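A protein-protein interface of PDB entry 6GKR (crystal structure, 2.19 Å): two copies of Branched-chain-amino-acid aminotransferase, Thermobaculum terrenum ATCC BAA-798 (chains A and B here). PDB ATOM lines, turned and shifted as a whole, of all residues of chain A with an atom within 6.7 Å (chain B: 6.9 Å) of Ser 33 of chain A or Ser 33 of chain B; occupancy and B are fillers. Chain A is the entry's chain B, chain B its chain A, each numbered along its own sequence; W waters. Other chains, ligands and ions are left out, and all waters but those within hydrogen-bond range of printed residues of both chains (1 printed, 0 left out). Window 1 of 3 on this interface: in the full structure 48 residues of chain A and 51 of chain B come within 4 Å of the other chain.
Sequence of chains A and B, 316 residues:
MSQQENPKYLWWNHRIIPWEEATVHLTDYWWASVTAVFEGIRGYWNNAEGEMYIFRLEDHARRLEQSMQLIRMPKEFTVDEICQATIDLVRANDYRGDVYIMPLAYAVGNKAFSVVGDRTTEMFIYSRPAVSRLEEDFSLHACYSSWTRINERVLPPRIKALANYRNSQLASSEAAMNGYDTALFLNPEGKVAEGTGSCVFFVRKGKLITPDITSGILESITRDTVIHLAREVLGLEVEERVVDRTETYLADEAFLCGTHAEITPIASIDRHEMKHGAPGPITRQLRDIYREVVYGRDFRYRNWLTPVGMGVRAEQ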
ATOM      1  N   TYR A  29     -20.272 -14.182   9.615  1.00  0.00           N
ATOM      2  CA  TYR A  29     -21.615 -14.375   9.076  1.00  0.00           C
ATOM      3  C   TYR A  29     -21.736 -15.435   7.978  1.00  0.00           C
ATOM      4  O   TYR A  29     -22.816 -15.576   7.417  1.00  0.00           O
ATOM      5  CB  TYR A  29     -22.221 -13.032   8.643  1.00  0.00           C
ATOM      6  CG  TYR A  29     -22.479 -12.160   9.841  1.00  0.00           C
ATOM      7  CD1 TYR A  29     -23.326 -12.588  10.853  1.00  0.00           C
ATOM      8  CD2 TYR A  29     -21.802 -10.960  10.011  1.00  0.00           C
ATOM      9  CE1 TYR A  29     -23.544 -11.806  11.979  1.00  0.00           C
ATOM     10  CE2 TYR A  29     -21.990 -10.181  11.145  1.00  0.00           C
ATOM     11  CZ  TYR A  29     -22.869 -10.602  12.130  1.00  0.00           C
ATOM     12  OH  TYR A  29     -23.070  -9.835  13.248  1.00  0.00           O
ATOM     13  N   TRP A  30     -20.663 -16.183   7.690  1.00  0.00           N
ATOM     14  CA  TRP A  30     -20.677 -17.127   6.576  1.00  0.00           C
ATOM     15  C   TRP A  30     -21.662 -18.291   6.806  1.00  0.00           C
ATOM     16  O   TRP A  30     -22.454 -18.618   5.922  1.00  0.00           O
ATOM     17  CB  TRP A  30     -19.257 -17.611   6.248  1.00  0.00           C
ATOM     18  CG  TRP A  30     -18.369 -16.484   5.825  1.00  0.00           C
ATOM     19  CD1 TRP A  30     -17.467 -15.816   6.608  1.00  0.00           C
ATOM     20  CD2 TRP A  30     -18.282 -15.889   4.513  1.00  0.00           C
ATOM     21  NE1 TRP A  30     -16.839 -14.844   5.878  1.00  0.00           N
ATOM     22  CE2 TRP A  30     -17.297 -14.880   4.589  1.00  0.00           C
ATOM     23  CE3 TRP A  30     -18.909 -16.131   3.283  1.00  0.00           C
ATOM     24  CZ2 TRP A  30     -16.963 -14.083   3.499  1.00  0.00           C
ATOM     25  CZ3 TRP A  30     -18.587 -15.338   2.204  1.00  0.00           C
ATOM     26  CH2 TRP A  30     -17.622 -14.334   2.312  1.00  0.00           C
ATOM     27  N   TRP A  31     -21.629 -18.892   7.994  1.00  0.00           N
ATOM     28  CA  TRP A  31     -22.569 -19.927   8.360  1.00  0.00           C
ATOM     29  C   TRP A  31     -23.970 -19.338   8.431  1.00  0.00           C
ATOM     30  O   TRP A  31     -24.919 -19.993   8.040  1.00  0.00           O
ATOM     31  CB  TRP A  31     -22.189 -20.586   9.686  1.00  0.00           C
ATOM     32  CG  TRP A  31     -20.792 -21.116   9.726  1.00  0.00           C
ATOM     33  CD1 TRP A  31     -20.356 -22.304   9.220  1.00  0.00           C
ATOM     34  CD2 TRP A  31     -19.638 -20.489  10.327  1.00  0.00           C
ATOM     35  NE1 TRP A  31     -19.015 -22.467   9.458  1.00  0.00           N
ATOM     36  CE2 TRP A  31     -18.543 -21.372  10.139  1.00  0.00           C
ATOM     37  CE3 TRP A  31     -19.419 -19.284  11.014  1.00  0.00           C
ATOM     38  CZ2 TRP A  31     -17.255 -21.071  10.601  1.00  0.00           C
ATOM     39  CZ3 TRP A  31     -18.148 -18.992  11.476  1.00  0.00           C
ATOM     40  CH2 TRP A  31     -17.085 -19.877  11.269  1.00  0.00           C
ATOM     41  N   ALA A  32     -24.098 -18.106   8.925  1.00  0.00           N
ATOM     42  CA  ALA A  32     -25.427 -17.524   9.086  1.00  0.00           C
ATOM     43  C   ALA A  32     -26.072 -17.311   7.715  1.00  0.00           C
ATOM     44  O   ALA A  32     -27.293 -17.374   7.599  1.00  0.00           O
ATOM     45  CB  ALA A  32     -25.360 -16.231   9.860  1.00  0.00           C
ATOM     46  N   SER A  33     -25.238 -17.059   6.685  1.00  0.00           N
ATOM     47  CA  SER A  33     -25.733 -16.698   5.368  1.00  0.00           C
ATOM     48  C   SER A  33     -26.535 -17.856   4.780  1.00  0.00           C
ATOM     49  O   SER A  33     -27.449 -17.624   4.011  1.00  0.00           O
ATOM     50  CB  SER A  33     -24.637 -16.272   4.443  1.00  0.00           C
ATOM     51  OG  SER A  33     -23.802 -17.381   4.129  1.00  0.00           O
ATOM     52  N   VAL A  34     -26.232 -19.087   5.196  1.00  0.00           N
ATOM     53  CA  VAL A  34     -26.964 -20.249   4.739  1.00  0.00           C
ATOM     54  C   VAL A  34     -28.409 -20.202   5.221  1.00  0.00           C
ATOM     55  O   VAL A  34     -29.267 -20.758   4.574  1.00  0.00           O
ATOM     56  CB  VAL A  34     -26.238 -21.524   5.188  1.00  0.00           C
ATOM     57  CG1 VAL A  34     -27.044 -22.804   4.963  1.00  0.00           C
ATOM     58  CG2 VAL A  34     -24.870 -21.576   4.517  1.00  0.00           C
ATOM     59  N   THR A  35     -28.680 -19.530   6.348  1.00  0.00           N
ATOM     60  CA  THR A  35     -30.026 -19.431   6.864  1.00  0.00           C
ATOM     61  C   THR A  35     -30.714 -18.179   6.340  1.00  0.00           C
ATOM     62  O   THR A  35     -31.894 -18.013   6.605  1.00  0.00           O
ATOM     63  CB  THR A  35     -30.054 -19.339   8.405  1.00  0.00           C
ATOM     64  OG1 THR A  35     -29.725 -17.993   8.797  1.00  0.00           O
ATOM     65  CG2 THR A  35     -29.137 -20.336   9.105  1.00  0.00           C
ATOM     66  N   ALA A  36     -29.980 -17.268   5.669  1.00  0.00           N
ATOM     67  CA  ALA A  36     -30.439 -15.908   5.475  1.00  0.00           C
ATOM     68  C   ALA A  36     -31.553 -15.808   4.437  1.00  0.00           C
ATOM     69  O   ALA A  36     -31.541 -16.475   3.408  1.00  0.00           O
ATOM     70  CB  ALA A  36     -29.281 -14.988   5.112  1.00  0.00           C
ATOM     71  N   VAL A  37     -32.481 -14.885   4.703  1.00  0.00           N
ATOM     72  CA  VAL A  37     -33.586 -14.528   3.823  1.00  0.00           C
ATOM     73  C   VAL A  37     -33.627 -13.006   3.742  1.00  0.00           C
ATOM     74  O   VAL A  37     -33.096 -12.329   4.629  1.00  0.00           O
ATOM     75  CB  VAL A  37     -34.933 -15.090   4.337  1.00  0.00           C
ATOM     76  CG1 VAL A  37     -34.909 -16.618   4.379  1.00  0.00           C
ATOM     77  CG2 VAL A  37     -35.329 -14.540   5.698  1.00  0.00           C
ATOM     78  N   LEU A 104     -32.641  -7.934   5.663  1.00  0.00           N
ATOM     79  CA  LEU A 104     -31.995  -9.236   5.549  1.00  0.00           C
ATOM     80  C   LEU A 104     -31.948  -9.851   6.952  1.00  0.00           C
ATOM     81  O   LEU A 104     -31.309  -9.286   7.838  1.00  0.00           O
ATOM     82  CB  LEU A 104     -30.572  -9.095   4.978  1.00  0.00           C
ATOM     83  CG  LEU A 104     -29.871 -10.428   4.651  1.00  0.00           C
ATOM     84  CD1 LEU A 104     -28.942 -10.327   3.442  1.00  0.00           C
ATOM     85  CD2 LEU A 104     -29.168 -11.054   5.857  1.00  0.00           C
ATOM     86  N   TYR A 106     -31.288 -13.353   9.514  1.00  0.00           N
ATOM     87  CA  TYR A 106     -30.381 -14.486   9.599  1.00  0.00           C
ATOM     88  C   TYR A 106     -30.467 -15.048  11.018  1.00  0.00           C
ATOM     89  O   TYR A 106     -30.750 -14.325  11.971  1.00  0.00           O
ATOM     90  CB  TYR A 106     -28.969 -14.079   9.158  1.00  0.00           C
ATOM     91  CG  TYR A 106     -28.356 -12.947   9.958  1.00  0.00           C
ATOM     92  CD1 TYR A 106     -28.602 -11.615   9.648  1.00  0.00           C
ATOM     93  CD2 TYR A 106     -27.572 -13.210  11.073  1.00  0.00           C
ATOM     94  CE1 TYR A 106     -28.097 -10.570  10.420  1.00  0.00           C
ATOM     95  CE2 TYR A 106     -27.055 -12.182  11.853  1.00  0.00           C
ATOM     96  CZ  TYR A 106     -27.310 -10.854  11.528  1.00  0.00           C
ATOM     97  OH  TYR A 106     -26.789  -9.840  12.300  1.00  0.00           O
ATOM     98  N   ALA A 107     -30.258 -16.350  11.163  1.00  0.00           N
ATOM     99  CA  ALA A 107     -30.177 -16.963  12.481  1.00  0.00           C
ATOM    100  C   ALA A 107     -28.717 -17.096  12.888  1.00  0.00           C
ATOM    101  O   ALA A 107     -27.913 -17.557  12.093  1.00  0.00           O
ATOM    102  CB  ALA A 107     -30.868 -18.315  12.502  1.00  0.00           C
ATOM    103  N   PHE A 113     -22.618 -25.209   9.217  1.00  0.00           N
ATOM    104  CA  PHE A 113     -23.569 -24.982   8.132  1.00  0.00           C
ATOM    105  C   PHE A 113     -24.690 -26.020   8.171  1.00  0.00           C
ATOM    106  O   PHE A 113     -25.859 -25.686   7.951  1.00  0.00           O
ATOM    107  CB  PHE A 113     -22.902 -25.167   6.767  1.00  0.00           C
ATOM    108  CG  PHE A 113     -21.702 -24.307   6.547  1.00  0.00           C
ATOM    109  CD1 PHE A 113     -21.863 -22.951   6.358  1.00  0.00           C
ATOM    110  CD2 PHE A 113     -20.428 -24.846   6.551  1.00  0.00           C
ATOM    111  CE1 PHE A 113     -20.758 -22.124   6.187  1.00  0.00           C
ATOM    112  CE2 PHE A 113     -19.319 -24.031   6.386  1.00  0.00           C
ATOM    113  CZ  PHE A 113     -19.486 -22.675   6.194  1.00  0.00           C
ATOM    114  N   ALA A 161     -34.692 -16.969   0.051  1.00  0.00           N
ATOM    115  CA  ALA A 161     -33.456 -17.312   0.738  1.00  0.00           C
ATOM    116  C   ALA A 161     -32.249 -16.929  -0.100  1.00  0.00           C
ATOM    117  O   ALA A 161     -32.244 -17.177  -1.285  1.00  0.00           O
ATOM    118  CB  ALA A 161     -33.428 -18.798   1.051  1.00  0.00           C
ATOM    119  N   LEU A 162     -31.179 -16.436   0.534  1.00  0.00           N
ATOM    120  CA  LEU A 162     -29.950 -16.154  -0.206  1.00  0.00           C
ATOM    121  C   LEU A 162     -29.473 -17.396  -0.964  1.00  0.00           C
ATOM    122  O   LEU A 162     -29.007 -17.279  -2.087  1.00  0.00           O
ATOM    123  CB  LEU A 162     -28.858 -15.706   0.766  1.00  0.00           C
ATOM    124  CG  LEU A 162     -28.574 -14.204   0.850  1.00  0.00           C
ATOM    125  CD1 LEU A 162     -29.773 -13.425   1.397  1.00  0.00           C
ATOM    126  CD2 LEU A 162     -27.357 -13.993   1.742  1.00  0.00           C
ATOM    127  N   ALA A 163     -29.606 -18.583  -0.373  1.00  0.00           N
ATOM    128  CA  ALA A 163     -29.019 -19.797  -0.936  1.00  0.00           C
ATOM    129  C   ALA A 163     -29.602 -20.112  -2.321  1.00  0.00           C
ATOM    130  O   ALA A 163     -28.907 -20.638  -3.174  1.00  0.00           O
ATOM    131  CB  ALA A 163     -29.248 -20.959   0.021  1.00  0.00           C
ATOM    132  N   ARG A 166     -27.733 -19.200  -5.580  1.00  0.00           N
ATOM    133  CA  ARG A 166     -26.646 -19.986  -6.142  1.00  0.00           C
ATOM    134  C   ARG A 166     -27.152 -20.636  -7.436  1.00  0.00           C
ATOM    135  O   ARG A 166     -26.444 -20.727  -8.434  1.00  0.00           O
ATOM    136  CB  ARG A 166     -26.149 -21.019  -5.124  1.00  0.00           C
ATOM    137  CG  ARG A 166     -25.181 -22.060  -5.669  1.00  0.00           C
ATOM    138  CD  ARG A 166     -23.726 -21.631  -5.597  1.00  0.00           C
ATOM    139  NE  ARG A 166     -23.373 -20.487  -6.476  1.00  0.00           N
ATOM    140  CZ  ARG A 166     -22.981 -20.596  -7.751  1.00  0.00           C
ATOM    141  NH1 ARG A 166     -22.872 -21.791  -8.328  1.00  0.00           N
ATOM    142  NH2 ARG A 166     -22.626 -19.513  -8.413  1.00  0.00           N
ATOM    143  N   GLN A 169     -27.432 -18.022 -10.070  1.00  0.00           N
ATOM    144  CA  GLN A 169     -26.095 -17.689 -10.561  1.00  0.00           C
ATOM    145  C   GLN A 169     -25.634 -18.671 -11.635  1.00  0.00           C
ATOM    146  O   GLN A 169     -24.933 -18.271 -12.543  1.00  0.00           O
ATOM    147  CB  GLN A 169     -25.076 -17.572  -9.422  1.00  0.00           C
ATOM    148  CG  GLN A 169     -25.251 -16.279  -8.620  1.00  0.00           C
ATOM    149  CD  GLN A 169     -24.206 -16.208  -7.533  1.00  0.00           C
ATOM    150  OE1 GLN A 169     -23.347 -17.100  -7.412  1.00  0.00           O
ATOM    151  NE2 GLN A 169     -24.326 -15.185  -6.689  1.00  0.00           N
ATOM    152  N   TYR B  29     -20.322  -8.862   2.918  1.00  0.00           N
ATOM    153  CA  TYR B  29     -20.076 -10.200   2.387  1.00  0.00           C
ATOM    154  C   TYR B  29     -21.336 -11.012   2.090  1.00  0.00           C
ATOM    155  O   TYR B  29     -21.222 -12.185   1.718  1.00  0.00           O
ATOM    156  CB  TYR B  29     -19.093 -10.974   3.273  1.00  0.00           C
ATOM    157  CG  TYR B  29     -17.727 -10.350   3.189  1.00  0.00           C
ATOM    158  CD1 TYR B  29     -17.079 -10.264   1.964  1.00  0.00           C
ATOM    159  CD2 TYR B  29     -17.130  -9.753   4.288  1.00  0.00           C
ATOM    160  CE1 TYR B  29     -15.847  -9.641   1.844  1.00  0.00           C
ATOM    161  CE2 TYR B  29     -15.907  -9.112   4.175  1.00  0.00           C
ATOM    162  CZ  TYR B  29     -15.261  -9.054   2.957  1.00  0.00           C
ATOM    163  OH  TYR B  29     -14.069  -8.403   2.852  1.00  0.00           O
ATOM    164  N   TRP B  30     -22.524 -10.392   2.213  1.00  0.00           N
ATOM    165  CA  TRP B  30     -23.770 -11.127   2.048  1.00  0.00           C
ATOM    166  C   TRP B  30     -23.956 -11.614   0.614  1.00  0.00           C
ATOM    167  O   TRP B  30     -24.276 -12.795   0.410  1.00  0.00           O
ATOM    168  CB  TRP B  30     -24.963 -10.316   2.565  1.00  0.00           C
ATOM    169  CG  TRP B  30     -24.870 -10.126   4.044  1.00  0.00           C
ATOM    170  CD1 TRP B  30     -24.416  -9.014   4.693  1.00  0.00           C
ATOM    171  CD2 TRP B  30     -25.202 -11.097   5.063  1.00  0.00           C
ATOM    172  NE1 TRP B  30     -24.429  -9.239   6.045  1.00  0.00           N
ATOM    173  CE2 TRP B  30     -24.886 -10.505   6.303  1.00  0.00           C
ATOM    174  CE3 TRP B  30     -25.756 -12.386   5.047  1.00  0.00           C
ATOM    175  CZ2 TRP B  30     -25.128 -11.150   7.515  1.00  0.00           C
ATOM    176  CZ3 TRP B  30     -25.949 -13.042   6.246  1.00  0.00           C
ATOM    177  CH2 TRP B  30     -25.635 -12.429   7.460  1.00  0.00           C
ATOM    178  N   TRP B  31     -23.736 -10.716  -0.369  1.00  0.00           N
ATOM    179  CA  TRP B  31     -23.856 -11.159  -1.751  1.00  0.00           C
ATOM    180  C   TRP B  31     -22.748 -12.151  -2.067  1.00  0.00           C
ATOM    181  O   TRP B  31     -22.987 -13.100  -2.808  1.00  0.00           O
ATOM    182  CB  TRP B  31     -23.860  -9.994  -2.735  1.00  0.00           C
ATOM    183  CG  TRP B  31     -24.883  -8.948  -2.406  1.00  0.00           C
ATOM    184  CD1 TRP B  31     -26.221  -8.979  -2.691  1.00  0.00           C
ATOM    185  CD2 TRP B  31     -24.623  -7.677  -1.782  1.00  0.00           C
ATOM    186  NE1 TRP B  31     -26.819  -7.822  -2.257  1.00  0.00           N
ATOM    187  CE2 TRP B  31     -25.869  -6.996  -1.701  1.00  0.00           C
ATOM    188  CE3 TRP B  31     -23.466  -7.039  -1.288  1.00  0.00           C
ATOM    189  CZ2 TRP B  31     -25.983  -5.725  -1.120  1.00  0.00           C
ATOM    190  CZ3 TRP B  31     -23.577  -5.772  -0.739  1.00  0.00           C
ATOM    191  CH2 TRP B  31     -24.826  -5.133  -0.642  1.00  0.00           C
ATOM    192  N   ALA B  32     -21.552 -11.934  -1.493  1.00  0.00           N
ATOM    193  CA  ALA B  32     -20.439 -12.822  -1.808  1.00  0.00           C
ATOM    194  C   ALA B  32     -20.721 -14.246  -1.322  1.00  0.00           C
ATOM    195  O   ALA B  32     -20.236 -15.209  -1.908  1.00  0.00           O
ATOM    196  CB  ALA B  32     -19.162 -12.281  -1.208  1.00  0.00           C
ATOM    197  N   SER B  33     -21.501 -14.365  -0.238  1.00  0.00           N
ATOM    198  CA  SER B  33     -21.719 -15.648   0.413  1.00  0.00           C
ATOM    199  C   SER B  33     -22.429 -16.615  -0.530  1.00  0.00           C
ATOM    200  O   SER B  33     -22.196 -17.818  -0.456  1.00  0.00           O
ATOM    201  CB  SER B  33     -22.487 -15.504   1.701  1.00  0.00           C
ATOM    202  OG  SER B  33     -23.810 -15.067   1.425  1.00  0.00           O
ATOM    203  N   VAL B  34     -23.217 -16.062  -1.457  1.00  0.00           N
ATOM    204  CA  VAL B  34     -23.932 -16.905  -2.400  1.00  0.00           C
ATOM    205  C   VAL B  34     -22.966 -17.614  -3.345  1.00  0.00           C
ATOM    206  O   VAL B  34     -23.282 -18.709  -3.830  1.00  0.00           O
ATOM    207  CB  VAL B  34     -25.020 -16.131  -3.164  1.00  0.00           C
ATOM    208  CG1 VAL B  34     -25.785 -17.063  -4.103  1.00  0.00           C
ATOM    209  CG2 VAL B  34     -25.955 -15.448  -2.183  1.00  0.00           C
ATOM    210  N   THR B  35     -21.797 -16.992  -3.577  1.00  0.00           N
ATOM    211  CA  THR B  35     -20.803 -17.557  -4.472  1.00  0.00           C
ATOM    212  C   THR B  35     -19.834 -18.473  -3.710  1.00  0.00           C
ATOM    213  O   THR B  35     -18.992 -19.102  -4.337  1.00  0.00           O
ATOM    214  CB  THR B  35     -19.932 -16.472  -5.134  1.00  0.00           C
ATOM    215  OG1 THR B  35     -18.919 -16.037  -4.213  1.00  0.00           O
ATOM    216  CG2 THR B  35     -20.731 -15.299  -5.677  1.00  0.00           C
ATOM    217  N   ALA B  36     -19.927 -18.522  -2.370  1.00  0.00           N
ATOM    218  CA  ALA B  36     -18.829 -19.040  -1.561  1.00  0.00           C
ATOM    219  C   ALA B  36     -18.716 -20.563  -1.616  1.00  0.00           C
ATOM    220  O   ALA B  36     -19.717 -21.275  -1.610  1.00  0.00           O
ATOM    221  CB  ALA B  36     -18.935 -18.543  -0.130  1.00  0.00           C
ATOM    222  N   VAL B  37     -17.471 -21.037  -1.628  1.00  0.00           N
ATOM    223  CA  VAL B  37     -17.126 -22.452  -1.544  1.00  0.00           C
ATOM    224  C   VAL B  37     -16.065 -22.618  -0.458  1.00  0.00           C
ATOM    225  O   VAL B  37     -15.342 -21.664  -0.156  1.00  0.00           O
ATOM    226  CB  VAL B  37     -16.615 -23.005  -2.894  1.00  0.00           C
ATOM    227  CG1 VAL B  37     -17.709 -22.895  -3.964  1.00  0.00           C
ATOM    228  CG2 VAL B  37     -15.348 -22.281  -3.363  1.00  0.00           C
ATOM    229  N   LEU B 104     -12.122 -20.709   2.914  1.00  0.00           N
ATOM    230  CA  LEU B 104     -13.371 -20.306   2.275  1.00  0.00           C
ATOM    231  C   LEU B 104     -13.066 -19.269   1.202  1.00  0.00           C
ATOM    232  O   LEU B 104     -12.489 -18.232   1.508  1.00  0.00           O
ATOM    233  CB  LEU B 104     -14.306 -19.714   3.330  1.00  0.00           C
ATOM    234  CG  LEU B 104     -15.734 -19.398   2.885  1.00  0.00           C
ATOM    235  CD1 LEU B 104     -16.710 -19.579   4.068  1.00  0.00           C
ATOM    236  CD2 LEU B 104     -15.835 -17.988   2.298  1.00  0.00           C
ATOM    237  N   ALA B 105     -13.406 -19.574  -0.058  1.00  0.00           N
ATOM    238  CA  ALA B 105     -13.201 -18.680  -1.199  1.00  0.00           C
ATOM    239  C   ALA B 105     -14.533 -18.042  -1.629  1.00  0.00           C
ATOM    240  O   ALA B 105     -15.594 -18.654  -1.524  1.00  0.00           O
ATOM    241  CB  ALA B 105     -12.595 -19.453  -2.326  1.00  0.00           C
ATOM    242  N   TYR B 106     -14.466 -16.807  -2.122  1.00  0.00           N
ATOM    243  CA  TYR B 106     -15.661 -16.063  -2.504  1.00  0.00           C
ATOM    244  C   TYR B 106     -15.293 -15.093  -3.622  1.00  0.00           C
ATOM    245  O   TYR B 106     -14.149 -14.648  -3.723  1.00  0.00           O
ATOM    246  CB  TYR B 106     -16.301 -15.399  -1.279  1.00  0.00           C
ATOM    247  CG  TYR B 106     -15.392 -14.458  -0.532  1.00  0.00           C
ATOM    248  CD1 TYR B 106     -14.495 -14.908   0.434  1.00  0.00           C
ATOM    249  CD2 TYR B 106     -15.375 -13.103  -0.850  1.00  0.00           C
ATOM    250  CE1 TYR B 106     -13.622 -14.033   1.072  1.00  0.00           C
ATOM    251  CE2 TYR B 106     -14.515 -12.214  -0.216  1.00  0.00           C
ATOM    252  CZ  TYR B 106     -13.648 -12.679   0.757  1.00  0.00           C
ATOM    253  OH  TYR B 106     -12.821 -11.770   1.354  1.00  0.00           O
ATOM    254  N   ALA B 107     -16.262 -14.814  -4.497  1.00  0.00           N
ATOM    255  CA  ALA B 107     -16.067 -13.809  -5.530  1.00  0.00           C
ATOM    256  C   ALA B 107     -16.580 -12.458  -5.054  1.00  0.00           C
ATOM    257  O   ALA B 107     -17.635 -12.398  -4.451  1.00  0.00           O
ATOM    258  CB  ALA B 107     -16.766 -14.225  -6.801  1.00  0.00           C
ATOM    259  N   PHE B 113     -27.395 -10.672  -5.786  1.00  0.00           N
ATOM    260  CA  PHE B 113     -27.364 -12.109  -5.542  1.00  0.00           C
ATOM    261  C   PHE B 113     -27.540 -12.906  -6.840  1.00  0.00           C
ATOM    262  O   PHE B 113     -26.881 -13.918  -7.050  1.00  0.00           O
ATOM    263  CB  PHE B 113     -28.492 -12.507  -4.591  1.00  0.00           C
ATOM    264  CG  PHE B 113     -28.463 -11.787  -3.273  1.00  0.00           C
ATOM    265  CD1 PHE B 113     -27.441 -12.023  -2.356  1.00  0.00           C
ATOM    266  CD2 PHE B 113     -29.421 -10.818  -2.978  1.00  0.00           C
ATOM    267  CE1 PHE B 113     -27.407 -11.334  -1.155  1.00  0.00           C
ATOM    268  CE2 PHE B 113     -29.376 -10.137  -1.772  1.00  0.00           C
ATOM    269  CZ  PHE B 113     -28.379 -10.406  -0.858  1.00  0.00           C
ATOM    270  N   ALA B 161     -20.254 -25.820  -2.061  1.00  0.00           N
ATOM    271  CA  ALA B 161     -20.757 -24.457  -1.959  1.00  0.00           C
ATOM    272  C   ALA B 161     -21.504 -24.249  -0.641  1.00  0.00           C
ATOM    273  O   ALA B 161     -22.263 -25.127  -0.213  1.00  0.00           O
ATOM    274  CB  ALA B 161     -21.684 -24.200  -3.126  1.00  0.00           C
ATOM    275  N   LEU B 162     -21.371 -23.064  -0.038  1.00  0.00           N
ATOM    276  CA  LEU B 162     -22.144 -22.762   1.164  1.00  0.00           C
ATOM    277  C   LEU B 162     -23.644 -22.945   0.904  1.00  0.00           C
ATOM    278  O   LEU B 162     -24.362 -23.453   1.759  1.00  0.00           O
ATOM    279  CB  LEU B 162     -21.845 -21.329   1.591  1.00  0.00           C
ATOM    280  CG  LEU B 162     -21.025 -21.117   2.866  1.00  0.00           C
ATOM    281  CD1 LEU B 162     -19.596 -21.636   2.695  1.00  0.00           C
ATOM    282  CD2 LEU B 162     -20.973 -19.623   3.178  1.00  0.00           C
ATOM    283  N   ALA B 163     -24.116 -22.556  -0.286  1.00  0.00           N
ATOM    284  CA  ALA B 163     -25.550 -22.517  -0.571  1.00  0.00           C
ATOM    285  C   ALA B 163     -26.188 -23.910  -0.431  1.00  0.00           C
ATOM    286  O   ALA B 163     -27.354 -24.024  -0.046  1.00  0.00           O
ATOM    287  CB  ALA B 163     -25.811 -21.884  -1.924  1.00  0.00           C
ATOM    288  N   ARG B 166     -28.230 -25.009   2.696  1.00  0.00           N
ATOM    289  CA  ARG B 166     -29.618 -24.647   2.956  1.00  0.00           C
ATOM    290  C   ARG B 166     -30.464 -25.908   2.799  1.00  0.00           C
ATOM    291  O   ARG B 166     -31.397 -26.133   3.555  1.00  0.00           O
ATOM    292  CB  ARG B 166     -30.058 -23.522   2.015  1.00  0.00           C
ATOM    293  CG  ARG B 166     -31.547 -23.223   2.032  1.00  0.00           C
ATOM    294  CD  ARG B 166     -32.025 -22.201   3.063  1.00  0.00           C
ATOM    295  NE  ARG B 166     -31.793 -22.630   4.443  1.00  0.00           N
ATOM    296  CZ  ARG B 166     -32.685 -23.255   5.199  1.00  0.00           C
ATOM    297  NH1 ARG B 166     -32.388 -23.561   6.461  1.00  0.00           N
ATOM    298  NH2 ARG B 166     -33.890 -23.535   4.699  1.00  0.00           N
HETATM  299  O   HOH W   1     -23.656 -12.852  -5.462  1.00  0.00           O
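The backbone carbonyl oxygen of Val 34 of chain B sits at hydrogen-bond distance from the guanidinium group of Arg 166 of chain A (3.2 Å). The side-chain amide nitrogen (NE2) of Gln 169 of chain A is in hydrogen-bond range of the backbone carbonyl oxygen (O) of Phe 113 of chain B, 2.9 Å away. The guanidinium group (NE) of Arg 166 of chain B lies within hydrogen-bond range of the backbone carbonyl oxygen (O) of Val 34 of chain A (3.1 Å).
O of Trp 30 of chain B is in hydrogen-bond range of OG of Ser 33 of chain B (2.5 Å). N of Leu 162 of chain B sits at hydrogen-bond distance from O of Ala 36 of chain B, 2.9 Å away. The side-chain hydroxyl (OG) of Ser 33 of chain A lies within hydrogen-bond range of the backbone carbonyl oxygen (O) of Trp 30 of chain A (2.6 Å).
Trp 30 of chain A touches Ala 36 of chain B. Trp 30 of chain B touches Leu 104 of chain A. CD2 of Leu 162 of chain A touches OG of Ser 33 of chain B, 3.7 Å away. Leu 162 of chain A touches Val 34 of chain B. Leu 162 of chain A touches Phe 113 of chain B. Ala 163 of chain B touches Ala 163 of chain A (CB to O, 3.6 Å). CB of Arg 166 of chain B touches CB of Ala 163 of chain A, at 3.3 Å. Thr 35 of chain B touches Gln 169 of chain A.
Printed residues of chain B within 4 Å of Tyr 29 of chain A: Trp 30 (3.6 Å). Of the printed residues of chain B, Trp 30 of chain A touches Tyr 29 (3.8 Å), Ser 33 (3.6 Å), Ala 36 (3.98 Å), Leu 104 (3.7 Å), Tyr 106 (3.6 Å) and Leu 162 (3.3 Å). Thr 35 of chain A touches none of the printed residues of chain B. Printed residues of chain B within 4 Å of Phe 113 of chain A: Leu 162. Trp 31 of chain B touches none of the printed residues of chain A. Ser 33 of chain B touches just these residues of chain A: Trp 30 (3.6 Å), Ser 33 (3.3 Å) and Leu 162 (3.7 Å). The nearest residue of chain A that does not touch Ser 33 of chain B is Tyr 29 of chain A (5.7 Å).
Of the 18 printed residues of chain A, 11 touch a printed residue of chain B. Hydrophobic or aromatic side chains of chain A within 4 Å of the printed part of chain B: Tyr 29, Trp 30, Val 34, Leu 104, Tyr 106, Phe 113, Leu 162 and Ala 163. Along chain A the printed residues that touch a printed residue of chain B span positions 29 to 169. Of the 18 printed residues of chain B, 12 touch a printed residue of chain A. Among the printed residues, 26 pairs touch across the chains. Among the printed residues, no Asp or Glu carboxylate lies within 4 Å of a Lys or Arg side-chain nitrogen of the other chain.
Trp 30 of chain A touches Ala 36 of chain B, but with the chains exchanged Ala 36 of chain A does not touch Trp 30 of chain B (4.02 Å). Trp 30 of chain A touches Leu 162 of chain B, and with the chains exchanged Leu 162 of chain A touches Trp 30 of chain B. Of the 26 pairs that touch across the chains among the printed residues, 22 have their exchanged pair printed and touching as well.
Water W1 lies within hydrogen-bond range of the side-chain amide nitrogen of Gln 169 of chain A (2.7 Å) and the backbone carbonyl oxygen of Trp 31 of chain B (2.7 Å).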
